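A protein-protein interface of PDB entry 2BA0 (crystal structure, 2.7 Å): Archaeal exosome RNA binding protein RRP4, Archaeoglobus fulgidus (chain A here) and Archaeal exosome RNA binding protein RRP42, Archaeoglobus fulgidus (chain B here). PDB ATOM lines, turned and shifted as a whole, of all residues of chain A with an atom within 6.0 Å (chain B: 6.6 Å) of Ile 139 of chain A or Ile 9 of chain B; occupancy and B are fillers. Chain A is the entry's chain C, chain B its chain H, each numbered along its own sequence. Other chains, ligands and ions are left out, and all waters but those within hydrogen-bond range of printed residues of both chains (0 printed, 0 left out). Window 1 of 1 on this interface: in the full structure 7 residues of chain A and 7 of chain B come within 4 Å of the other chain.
OH of Tyr 78 of chain A touches C of Ile 5 of chain B (3.6 Å).
Arg 138 of chain A touches Asp 12 of chain B.
O of Ile 139 of chain A touches CG2 of Ile 9 of chain B, at 3.6 Å.
Leu 6 of chain B touches Ala 141 of chain A.
Ala 141 of chain A touches Ile 9 of chain B.
CD2 of Leu 176 of chain A touches CD1 of Ile 9 of chain B, 3.9 Å away.
CD of Glu 190 of chain A touches CE2 of Tyr 13 of chain B (3.8 Å).
CE of Lys 10 of chain B touches CE2 of Tyr 194 of chain A, 3.7 Å away.
Tyr 194 of chain A touches Tyr 13 of chain B (CE1 to CE1, 3.5 Å).
Hydrophobic or aromatic side chains of chain A within 4 Å of the printed part of chain B: Tyr 78, Ala 141, Leu 176 and Tyr 194.
The backbone carbonyl oxygen of Val 179 of chain A lies within hydrogen-bond range of the backbone NH of Arg 138 of chain A, at 2.8 Å.
Printed residues of chain B within 4 Å of Ile 139 of chain A: Ile 9.
Ile 9 of chain B touches just these residues of chain A: Ile 139, Ala 141 and Leu 176.
Of the printed residues of chain B, Tyr 78 of chain A touches Ile 5 (3.6 Å) and Leu 6 (3.1 Å).
Of the printed residues of chain B, Ala 141 of chain A touches Leu 6 and Ile 9.
Asp 8 of chain B touches none of the printed residues of chain A.
The nearest printed residue of chain B that does not touch Ile 139 of chain A is Lys 10 of chain B (6.2 Å).
The nearest printed residue of chain B that does not touch Tyr 78 of chain A is Ile 9 of chain B (4.2 Å).
OH of Tyr 78 of chain A lies within hydrogen-bond range of N of Leu 6 of chain B (3.1 Å).
The backbone NH of Tyr 13 of chain B sits close to the guanidinium group of Arg 138 of chain A, at 3.4 Å.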
ATOM      1  N   ILE A  62      24.343 -30.453  16.528  1.00  0.00           N
ATOM      2  CA  ILE A  62      22.947 -30.151  16.822  1.00  0.00           C
ATOM      3  C   ILE A  62      22.188 -31.468  16.819  1.00  0.00           C
ATOM      4  O   ILE A  62      22.070 -32.117  15.781  1.00  0.00           O
ATOM      5  CB  ILE A  62      22.326 -29.221  15.773  1.00  0.00           C
ATOM      6  CG1 ILE A  62      22.727 -27.775  16.067  1.00  0.00           C
ATOM      7  CG2 ILE A  62      20.815 -29.361  15.778  1.00  0.00           C
ATOM      8  CD1 ILE A  62      22.152 -26.766  15.082  1.00  0.00           C
ATOM      9  N   ILE A  64      18.801 -34.076  18.559  1.00  0.00           N
ATOM     10  CA  ILE A  64      17.382 -34.083  18.898  1.00  0.00           C
ATOM     11  C   ILE A  64      17.127 -35.121  19.975  1.00  0.00           C
ATOM     12  O   ILE A  64      17.677 -36.213  19.922  1.00  0.00           O
ATOM     13  CB  ILE A  64      16.520 -34.432  17.681  1.00  0.00           C
ATOM     14  CG1 ILE A  64      16.758 -33.409  16.572  1.00  0.00           C
ATOM     15  CG2 ILE A  64      15.057 -34.448  18.074  1.00  0.00           C
ATOM     16  CD1 ILE A  64      15.981 -33.683  15.301  1.00  0.00           C
ATOM     17  N   TYR A  78      22.537 -37.916  14.365  1.00  0.00           N
ATOM     18  CA  TYR A  78      22.563 -38.338  12.974  1.00  0.00           C
ATOM     19  C   TYR A  78      23.936 -38.846  12.528  1.00  0.00           C
ATOM     20  O   TYR A  78      24.650 -38.190  11.765  1.00  0.00           O
ATOM     21  CB  TYR A  78      22.076 -37.180  12.095  1.00  0.00           C
ATOM     22  CG  TYR A  78      20.615 -36.818  12.348  1.00  0.00           C
ATOM     23  CD1 TYR A  78      20.042 -35.680  11.771  1.00  0.00           C
ATOM     24  CD2 TYR A  78      19.791 -37.641  13.133  1.00  0.00           C
ATOM     25  CE1 TYR A  78      18.685 -35.366  11.973  1.00  0.00           C
ATOM     26  CE2 TYR A  78      18.436 -37.336  13.340  1.00  0.00           C
ATOM     27  CZ  TYR A  78      17.890 -36.200  12.749  1.00  0.00           C
ATOM     28  OH  TYR A  78      16.553 -35.902  12.916  1.00  0.00           O
ATOM     29  N   ALA A 108      15.133 -30.138  20.253  1.00  0.00           N
ATOM     30  CA  ALA A 108      16.400 -29.974  19.545  1.00  0.00           C
ATOM     31  C   ALA A 108      17.387 -29.185  20.403  1.00  0.00           C
ATOM     32  O   ALA A 108      17.074 -28.097  20.901  1.00  0.00           O
ATOM     33  CB  ALA A 108      16.172 -29.255  18.215  1.00  0.00           C
ATOM     34  N   ILE A 134      17.324 -25.412  21.762  1.00  0.00           N
ATOM     35  CA  ILE A 134      16.698 -24.641  20.702  1.00  0.00           C
ATOM     36  C   ILE A 134      15.184 -24.628  20.866  1.00  0.00           C
ATOM     37  O   ILE A 134      14.557 -25.675  21.031  1.00  0.00           O
ATOM     38  CB  ILE A 134      17.065 -25.205  19.309  1.00  0.00           C
ATOM     39  CG1 ILE A 134      18.572 -25.073  19.086  1.00  0.00           C
ATOM     40  CG2 ILE A 134      16.308 -24.460  18.218  1.00  0.00           C
ATOM     41  CD1 ILE A 134      19.045 -25.574  17.753  1.00  0.00           C
ATOM     42  N   PHE A 136      13.655 -21.615  19.237  1.00  0.00           N
ATOM     43  CA  PHE A 136      13.466 -20.435  18.399  1.00  0.00           C
ATOM     44  C   PHE A 136      14.096 -20.632  17.021  1.00  0.00           C
ATOM     45  O   PHE A 136      14.761 -21.634  16.771  1.00  0.00           O
ATOM     46  CB  PHE A 136      14.106 -19.215  19.068  1.00  0.00           C
ATOM     47  CG  PHE A 136      13.188 -18.474  19.980  1.00  0.00           C
ATOM     48  CD1 PHE A 136      12.335 -17.499  19.476  1.00  0.00           C
ATOM     49  CD2 PHE A 136      13.152 -18.766  21.339  1.00  0.00           C
ATOM     50  CE1 PHE A 136      11.453 -16.820  20.312  1.00  0.00           C
ATOM     51  CE2 PHE A 136      12.272 -18.095  22.189  1.00  0.00           C
ATOM     52  CZ  PHE A 136      11.419 -17.118  21.672  1.00  0.00           C
ATOM     53  N   GLY A 137      13.883 -19.668  16.132  1.00  0.00           N
ATOM     54  CA  GLY A 137      14.459 -19.746  14.803  1.00  0.00           C
ATOM     55  C   GLY A 137      14.072 -20.954  13.966  1.00  0.00           C
ATOM     56  O   GLY A 137      12.964 -21.484  14.080  1.00  0.00           O
ATOM     57  N   ARG A 138      14.989 -21.378  13.100  1.00  0.00           N
ATOM     58  CA  ARG A 138      14.749 -22.525  12.236  1.00  0.00           C
ATOM     59  C   ARG A 138      15.985 -23.390  12.103  1.00  0.00           C
ATOM     60  O   ARG A 138      17.107 -22.929  12.318  1.00  0.00           O
ATOM     61  CB  ARG A 138      14.305 -22.080  10.843  1.00  0.00           C
ATOM     62  CG  ARG A 138      12.967 -21.376  10.801  1.00  0.00           C
ATOM     63  CD  ARG A 138      12.330 -21.570   9.440  1.00  0.00           C
ATOM     64  NE  ARG A 138      12.104 -22.991   9.189  1.00  0.00           N
ATOM     65  CZ  ARG A 138      11.632 -23.495   8.053  1.00  0.00           C
ATOM     66  NH1 ARG A 138      11.329 -22.693   7.041  1.00  0.00           N
ATOM     67  NH2 ARG A 138      11.465 -24.803   7.934  1.00  0.00           N
ATOM     68  N   ILE A 139      15.766 -24.651  11.741  1.00  0.00           N
ATOM     69  CA  ILE A 139      16.849 -25.604  11.564  1.00  0.00           C
ATOM     70  C   ILE A 139      16.957 -26.065  10.111  1.00  0.00           C
ATOM     71  O   ILE A 139      15.974 -26.508   9.512  1.00  0.00           O
ATOM     72  CB  ILE A 139      16.651 -26.860  12.443  1.00  0.00           C
ATOM     73  CG1 ILE A 139      16.617 -26.479  13.924  1.00  0.00           C
ATOM     74  CG2 ILE A 139      17.780 -27.850  12.189  1.00  0.00           C
ATOM     75  CD1 ILE A 139      16.457 -27.671  14.855  1.00  0.00           C
ATOM     76  N   VAL A 140      18.149 -25.955   9.538  1.00  0.00           N
ATOM     77  CA  VAL A 140      18.352 -26.416   8.171  1.00  0.00           C
ATOM     78  C   VAL A 140      19.291 -27.618   8.268  1.00  0.00           C
ATOM     79  O   VAL A 140      20.167 -27.648   9.131  1.00  0.00           O
ATOM     80  CB  VAL A 140      18.986 -25.316   7.273  1.00  0.00           C
ATOM     81  CG1 VAL A 140      18.718 -23.944   7.871  1.00  0.00           C
ATOM     82  CG2 VAL A 140      20.478 -25.566   7.089  1.00  0.00           C
ATOM     83  N   ALA A 141      19.095 -28.614   7.408  1.00  0.00           N
ATOM     84  CA  ALA A 141      19.942 -29.804   7.421  1.00  0.00           C
ATOM     85  C   ALA A 141      20.584 -30.037   6.057  1.00  0.00           C
ATOM     86  O   ALA A 141      19.892 -30.182   5.044  1.00  0.00           O
ATOM     87  CB  ALA A 141      19.130 -31.023   7.836  1.00  0.00           C
ATOM     88  N   LEU A 176      23.678 -30.316  10.781  1.00  0.00           N
ATOM     89  CA  LEU A 176      22.490 -29.586  11.211  1.00  0.00           C
ATOM     90  C   LEU A 176      22.847 -28.157  11.603  1.00  0.00           C
ATOM     91  O   LEU A 176      23.682 -27.925  12.474  1.00  0.00           O
ATOM     92  CB  LEU A 176      21.806 -30.322  12.367  1.00  0.00           C
ATOM     93  CG  LEU A 176      21.349 -31.745  12.024  1.00  0.00           C
ATOM     94  CD1 LEU A 176      20.501 -32.294  13.150  1.00  0.00           C
ATOM     95  CD2 LEU A 176      20.540 -31.735  10.736  1.00  0.00           C
ATOM     96  N   ILE A 177      22.204 -27.200  10.949  1.00  0.00           N
ATOM     97  CA  ILE A 177      22.483 -25.797  11.194  1.00  0.00           C
ATOM     98  C   ILE A 177      21.309 -25.054  11.804  1.00  0.00           C
ATOM     99  O   ILE A 177      20.168 -25.253  11.396  1.00  0.00           O
ATOM    100  CB  ILE A 177      22.867 -25.084   9.874  1.00  0.00           C
ATOM    101  CG1 ILE A 177      24.011 -25.834   9.183  1.00  0.00           C
ATOM    102  CG2 ILE A 177      23.284 -23.651  10.163  1.00  0.00           C
ATOM    103  CD1 ILE A 177      24.377 -25.278   7.821  1.00  0.00           C
ATOM    104  N   TRP A 178      21.592 -24.199  12.784  1.00  0.00           N
ATOM    105  CA  TRP A 178      20.543 -23.395  13.412  1.00  0.00           C
ATOM    106  C   TRP A 178      20.643 -21.955  12.937  1.00  0.00           C
ATOM    107  O   TRP A 178      21.724 -21.361  12.935  1.00  0.00           O
ATOM    108  CB  TRP A 178      20.642 -23.406  14.942  1.00  0.00           C
ATOM    109  CG  TRP A 178      19.615 -22.504  15.588  1.00  0.00           C
ATOM    110  CD1 TRP A 178      18.265 -22.523  15.377  1.00  0.00           C
ATOM    111  CD2 TRP A 178      19.856 -21.448  16.535  1.00  0.00           C
ATOM    112  NE1 TRP A 178      17.652 -21.547  16.128  1.00  0.00           N
ATOM    113  CE2 TRP A 178      18.601 -20.877  16.848  1.00  0.00           C
ATOM    114  CE3 TRP A 178      21.005 -20.935  17.147  1.00  0.00           C
ATOM    115  CZ2 TRP A 178      18.468 -19.814  17.750  1.00  0.00           C
ATOM    116  CZ3 TRP A 178      20.867 -19.874  18.046  1.00  0.00           C
ATOM    117  CH2 TRP A 178      19.605 -19.330  18.338  1.00  0.00           C
ATOM    118  N   VAL A 179      19.505 -21.406  12.530  1.00  0.00           N
ATOM    119  CA  VAL A 179      19.433 -20.033  12.058  1.00  0.00           C
ATOM    120  C   VAL A 179      18.366 -19.301  12.872  1.00  0.00           C
ATOM    121  O   VAL A 179      17.321 -19.876  13.189  1.00  0.00           O
ATOM    122  CB  VAL A 179      19.062 -19.985  10.558  1.00  0.00           C
ATOM    123  CG1 VAL A 179      18.966 -18.549  10.092  1.00  0.00           C
ATOM    124  CG2 VAL A 179      20.106 -20.731   9.742  1.00  0.00           C
ATOM    125  N   GLU A 190      18.375 -19.244   4.721  1.00  0.00           N
ATOM    126  CA  GLU A 190      18.013 -20.644   4.616  1.00  0.00           C
ATOM    127  C   GLU A 190      18.193 -21.036   3.146  1.00  0.00           C
ATOM    128  O   GLU A 190      18.983 -21.921   2.814  1.00  0.00           O
ATOM    129  CB  GLU A 190      16.555 -20.802   5.053  1.00  0.00           C
ATOM    130  CG  GLU A 190      16.125 -22.201   5.440  1.00  0.00           C
ATOM    131  CD  GLU A 190      14.697 -22.242   5.972  1.00  0.00           C
ATOM    132  N   TYR A 194      20.959 -23.789   1.236  1.00  0.00           N
ATOM    133  CA  TYR A 194      20.543 -24.925   0.426  1.00  0.00           C
ATOM    134  C   TYR A 194      21.105 -24.827  -0.985  1.00  0.00           C
ATOM    135  O   TYR A 194      21.578 -25.823  -1.536  1.00  0.00           O
ATOM    136  CB  TYR A 194      19.012 -25.012   0.380  1.00  0.00           C
ATOM    137  CG  TYR A 194      18.399 -25.605   1.628  1.00  0.00           C
ATOM    138  CD1 TYR A 194      17.236 -25.064   2.187  1.00  0.00           C
ATOM    139  CD2 TYR A 194      18.986 -26.699   2.264  1.00  0.00           C
ATOM    140  CE1 TYR A 194      16.675 -25.599   3.341  1.00  0.00           C
ATOM    141  CE2 TYR A 194      18.431 -27.240   3.422  1.00  0.00           C
ATOM    142  CZ  TYR A 194      17.282 -26.683   3.959  1.00  0.00           C
ATOM    143  OH  TYR A 194      16.757 -27.199   5.126  1.00  0.00           O
ATOM    144  N   ILE B   5      13.221 -37.638  12.260  1.00  0.00           N
ATOM    145  CA  ILE B   5      12.880 -36.223  12.239  1.00  0.00           C
ATOM    146  C   ILE B   5      13.541 -35.532  11.049  1.00  0.00           C
ATOM    147  O   ILE B   5      13.086 -34.472  10.617  1.00  0.00           O
ATOM    148  N   LEU B   6      14.614 -36.126  10.523  1.00  0.00           N
ATOM    149  CA  LEU B   6      15.311 -35.548   9.373  1.00  0.00           C
ATOM    150  C   LEU B   6      14.302 -35.326   8.252  1.00  0.00           C
ATOM    151  O   LEU B   6      14.486 -34.470   7.382  1.00  0.00           O
ATOM    152  CB  LEU B   6      16.431 -36.473   8.892  1.00  0.00           C
ATOM    153  CG  LEU B   6      17.274 -35.984   7.705  1.00  0.00           C
ATOM    154  CD1 LEU B   6      16.501 -36.102   6.395  1.00  0.00           C
ATOM    155  CD2 LEU B   6      17.703 -34.548   7.958  1.00  0.00           C
ATOM    156  N   VAL B   7      13.243 -36.124   8.272  1.00  0.00           N
ATOM    157  CA  VAL B   7      12.187 -35.988   7.292  1.00  0.00           C
ATOM    158  C   VAL B   7      11.426 -34.744   7.736  1.00  0.00           C
ATOM    159  O   VAL B   7      11.102 -33.884   6.919  1.00  0.00           O
ATOM    160  CB  VAL B   7      11.238 -37.210   7.304  1.00  0.00           C
ATOM    161  N   ASP B   8      11.174 -34.647   9.043  1.00  0.00           N
ATOM    162  CA  ASP B   8      10.455 -33.510   9.617  1.00  0.00           C
ATOM    163  C   ASP B   8      11.205 -32.197   9.446  1.00  0.00           C
ATOM    164  O   ASP B   8      10.591 -31.136   9.375  1.00  0.00           O
ATOM    165  N   ILE B   9      12.532 -32.258   9.387  1.00  0.00           N
ATOM    166  CA  ILE B   9      13.301 -31.037   9.198  1.00  0.00           C
ATOM    167  C   ILE B   9      12.991 -30.474   7.819  1.00  0.00           C
ATOM    168  O   ILE B   9      12.667 -29.296   7.681  1.00  0.00           O
ATOM    169  CB  ILE B   9      14.807 -31.279   9.315  1.00  0.00           C
ATOM    170  CG1 ILE B   9      15.166 -31.581  10.770  1.00  0.00           C
ATOM    171  CG2 ILE B   9      15.567 -30.052   8.838  1.00  0.00           C
ATOM    172  CD1 ILE B   9      16.644 -31.794  11.009  1.00  0.00           C
ATOM    173  N   LYS B  10      13.081 -31.314   6.795  1.00  0.00           N
ATOM    174  CA  LYS B  10      12.768 -30.855   5.458  1.00  0.00           C
ATOM    175  C   LYS B  10      11.268 -30.903   5.216  1.00  0.00           C
ATOM    176  O   LYS B  10      10.765 -30.338   4.251  1.00  0.00           O
ATOM    177  CB  LYS B  10      13.516 -31.673   4.410  1.00  0.00           C
ATOM    178  CG  LYS B  10      14.931 -31.177   4.215  1.00  0.00           C
ATOM    179  CD  LYS B  10      15.336 -31.219   2.765  1.00  0.00           C
ATOM    180  CE  LYS B  10      16.436 -30.207   2.493  1.00  0.00           C
ATOM    181  NZ  LYS B  10      16.953 -30.280   1.100  1.00  0.00           N
ATOM    182  N   ARG B  11      10.550 -31.581   6.096  1.00  0.00           N
ATOM    183  CA  ARG B  11       9.107 -31.649   5.974  1.00  0.00           C
ATOM    184  C   ARG B  11       8.623 -30.265   6.376  1.00  0.00           C
ATOM    185  O   ARG B  11       7.708 -29.714   5.766  1.00  0.00           O
ATOM    186  CB  ARG B  11       8.534 -32.694   6.927  1.00  0.00           C
ATOM    187  CG  ARG B  11       7.025 -32.784   6.909  1.00  0.00           C
ATOM    188  CD  ARG B  11       6.501 -33.702   7.998  1.00  0.00           C
ATOM    189  NE  ARG B  11       5.057 -33.854   7.882  1.00  0.00           N
ATOM    190  CZ  ARG B  11       4.289 -34.481   8.768  1.00  0.00           C
ATOM    191  NH1 ARG B  11       2.978 -34.568   8.565  1.00  0.00           N
ATOM    192  NH2 ARG B  11       4.828 -35.011   9.863  1.00  0.00           N
ATOM    193  N   ASP B  12       9.262 -29.706   7.405  1.00  0.00           N
ATOM    194  CA  ASP B  12       8.920 -28.379   7.908  1.00  0.00           C
ATOM    195  C   ASP B  12       9.227 -27.312   6.884  1.00  0.00           C
ATOM    196  O   ASP B  12       8.464 -26.372   6.721  1.00  0.00           O
ATOM    197  CB  ASP B  12       9.673 -28.081   9.207  1.00  0.00           C
ATOM    198  CG  ASP B  12       8.996 -28.693  10.431  1.00  0.00           C
ATOM    199  N   TYR B  13      10.348 -27.461   6.192  1.00  0.00           N
ATOM    200  CA  TYR B  13      10.745 -26.511   5.160  1.00  0.00           C
ATOM    201  C   TYR B  13       9.697 -26.531   4.042  1.00  0.00           C
ATOM    202  O   TYR B  13       9.169 -25.488   3.659  1.00  0.00           O
ATOM    203  CB  TYR B  13      12.122 -26.899   4.603  1.00  0.00           C
ATOM    204  CG  TYR B  13      12.689 -25.964   3.555  1.00  0.00           C
ATOM    205  CD1 TYR B  13      13.225 -26.467   2.369  1.00  0.00           C
ATOM    206  CD2 TYR B  13      12.724 -24.585   3.760  1.00  0.00           C
ATOM    207  CE1 TYR B  13      13.783 -25.625   1.412  1.00  0.00           C
ATOM    208  CE2 TYR B  13      13.279 -23.729   2.815  1.00  0.00           C
ATOM    209  CZ  TYR B  13      13.805 -24.259   1.644  1.00  0.00           C
ATOM    210  OH  TYR B  13      14.355 -23.427   0.703  1.00  0.00           O
ATOM    211  N   VAL B  14       9.399 -27.720   3.524  1.00  0.00           N
ATOM    212  CA  VAL B  14       8.409 -27.857   2.464  1.00  0.00           C
ATOM    213  C   VAL B  14       7.094 -27.232   2.907  1.00  0.00           C
ATOM    214  O   VAL B  14       6.500 -26.445   2.176  1.00  0.00           O
ATOM    215  CB  VAL B  14       8.165 -29.345   2.085  1.00  0.00           C
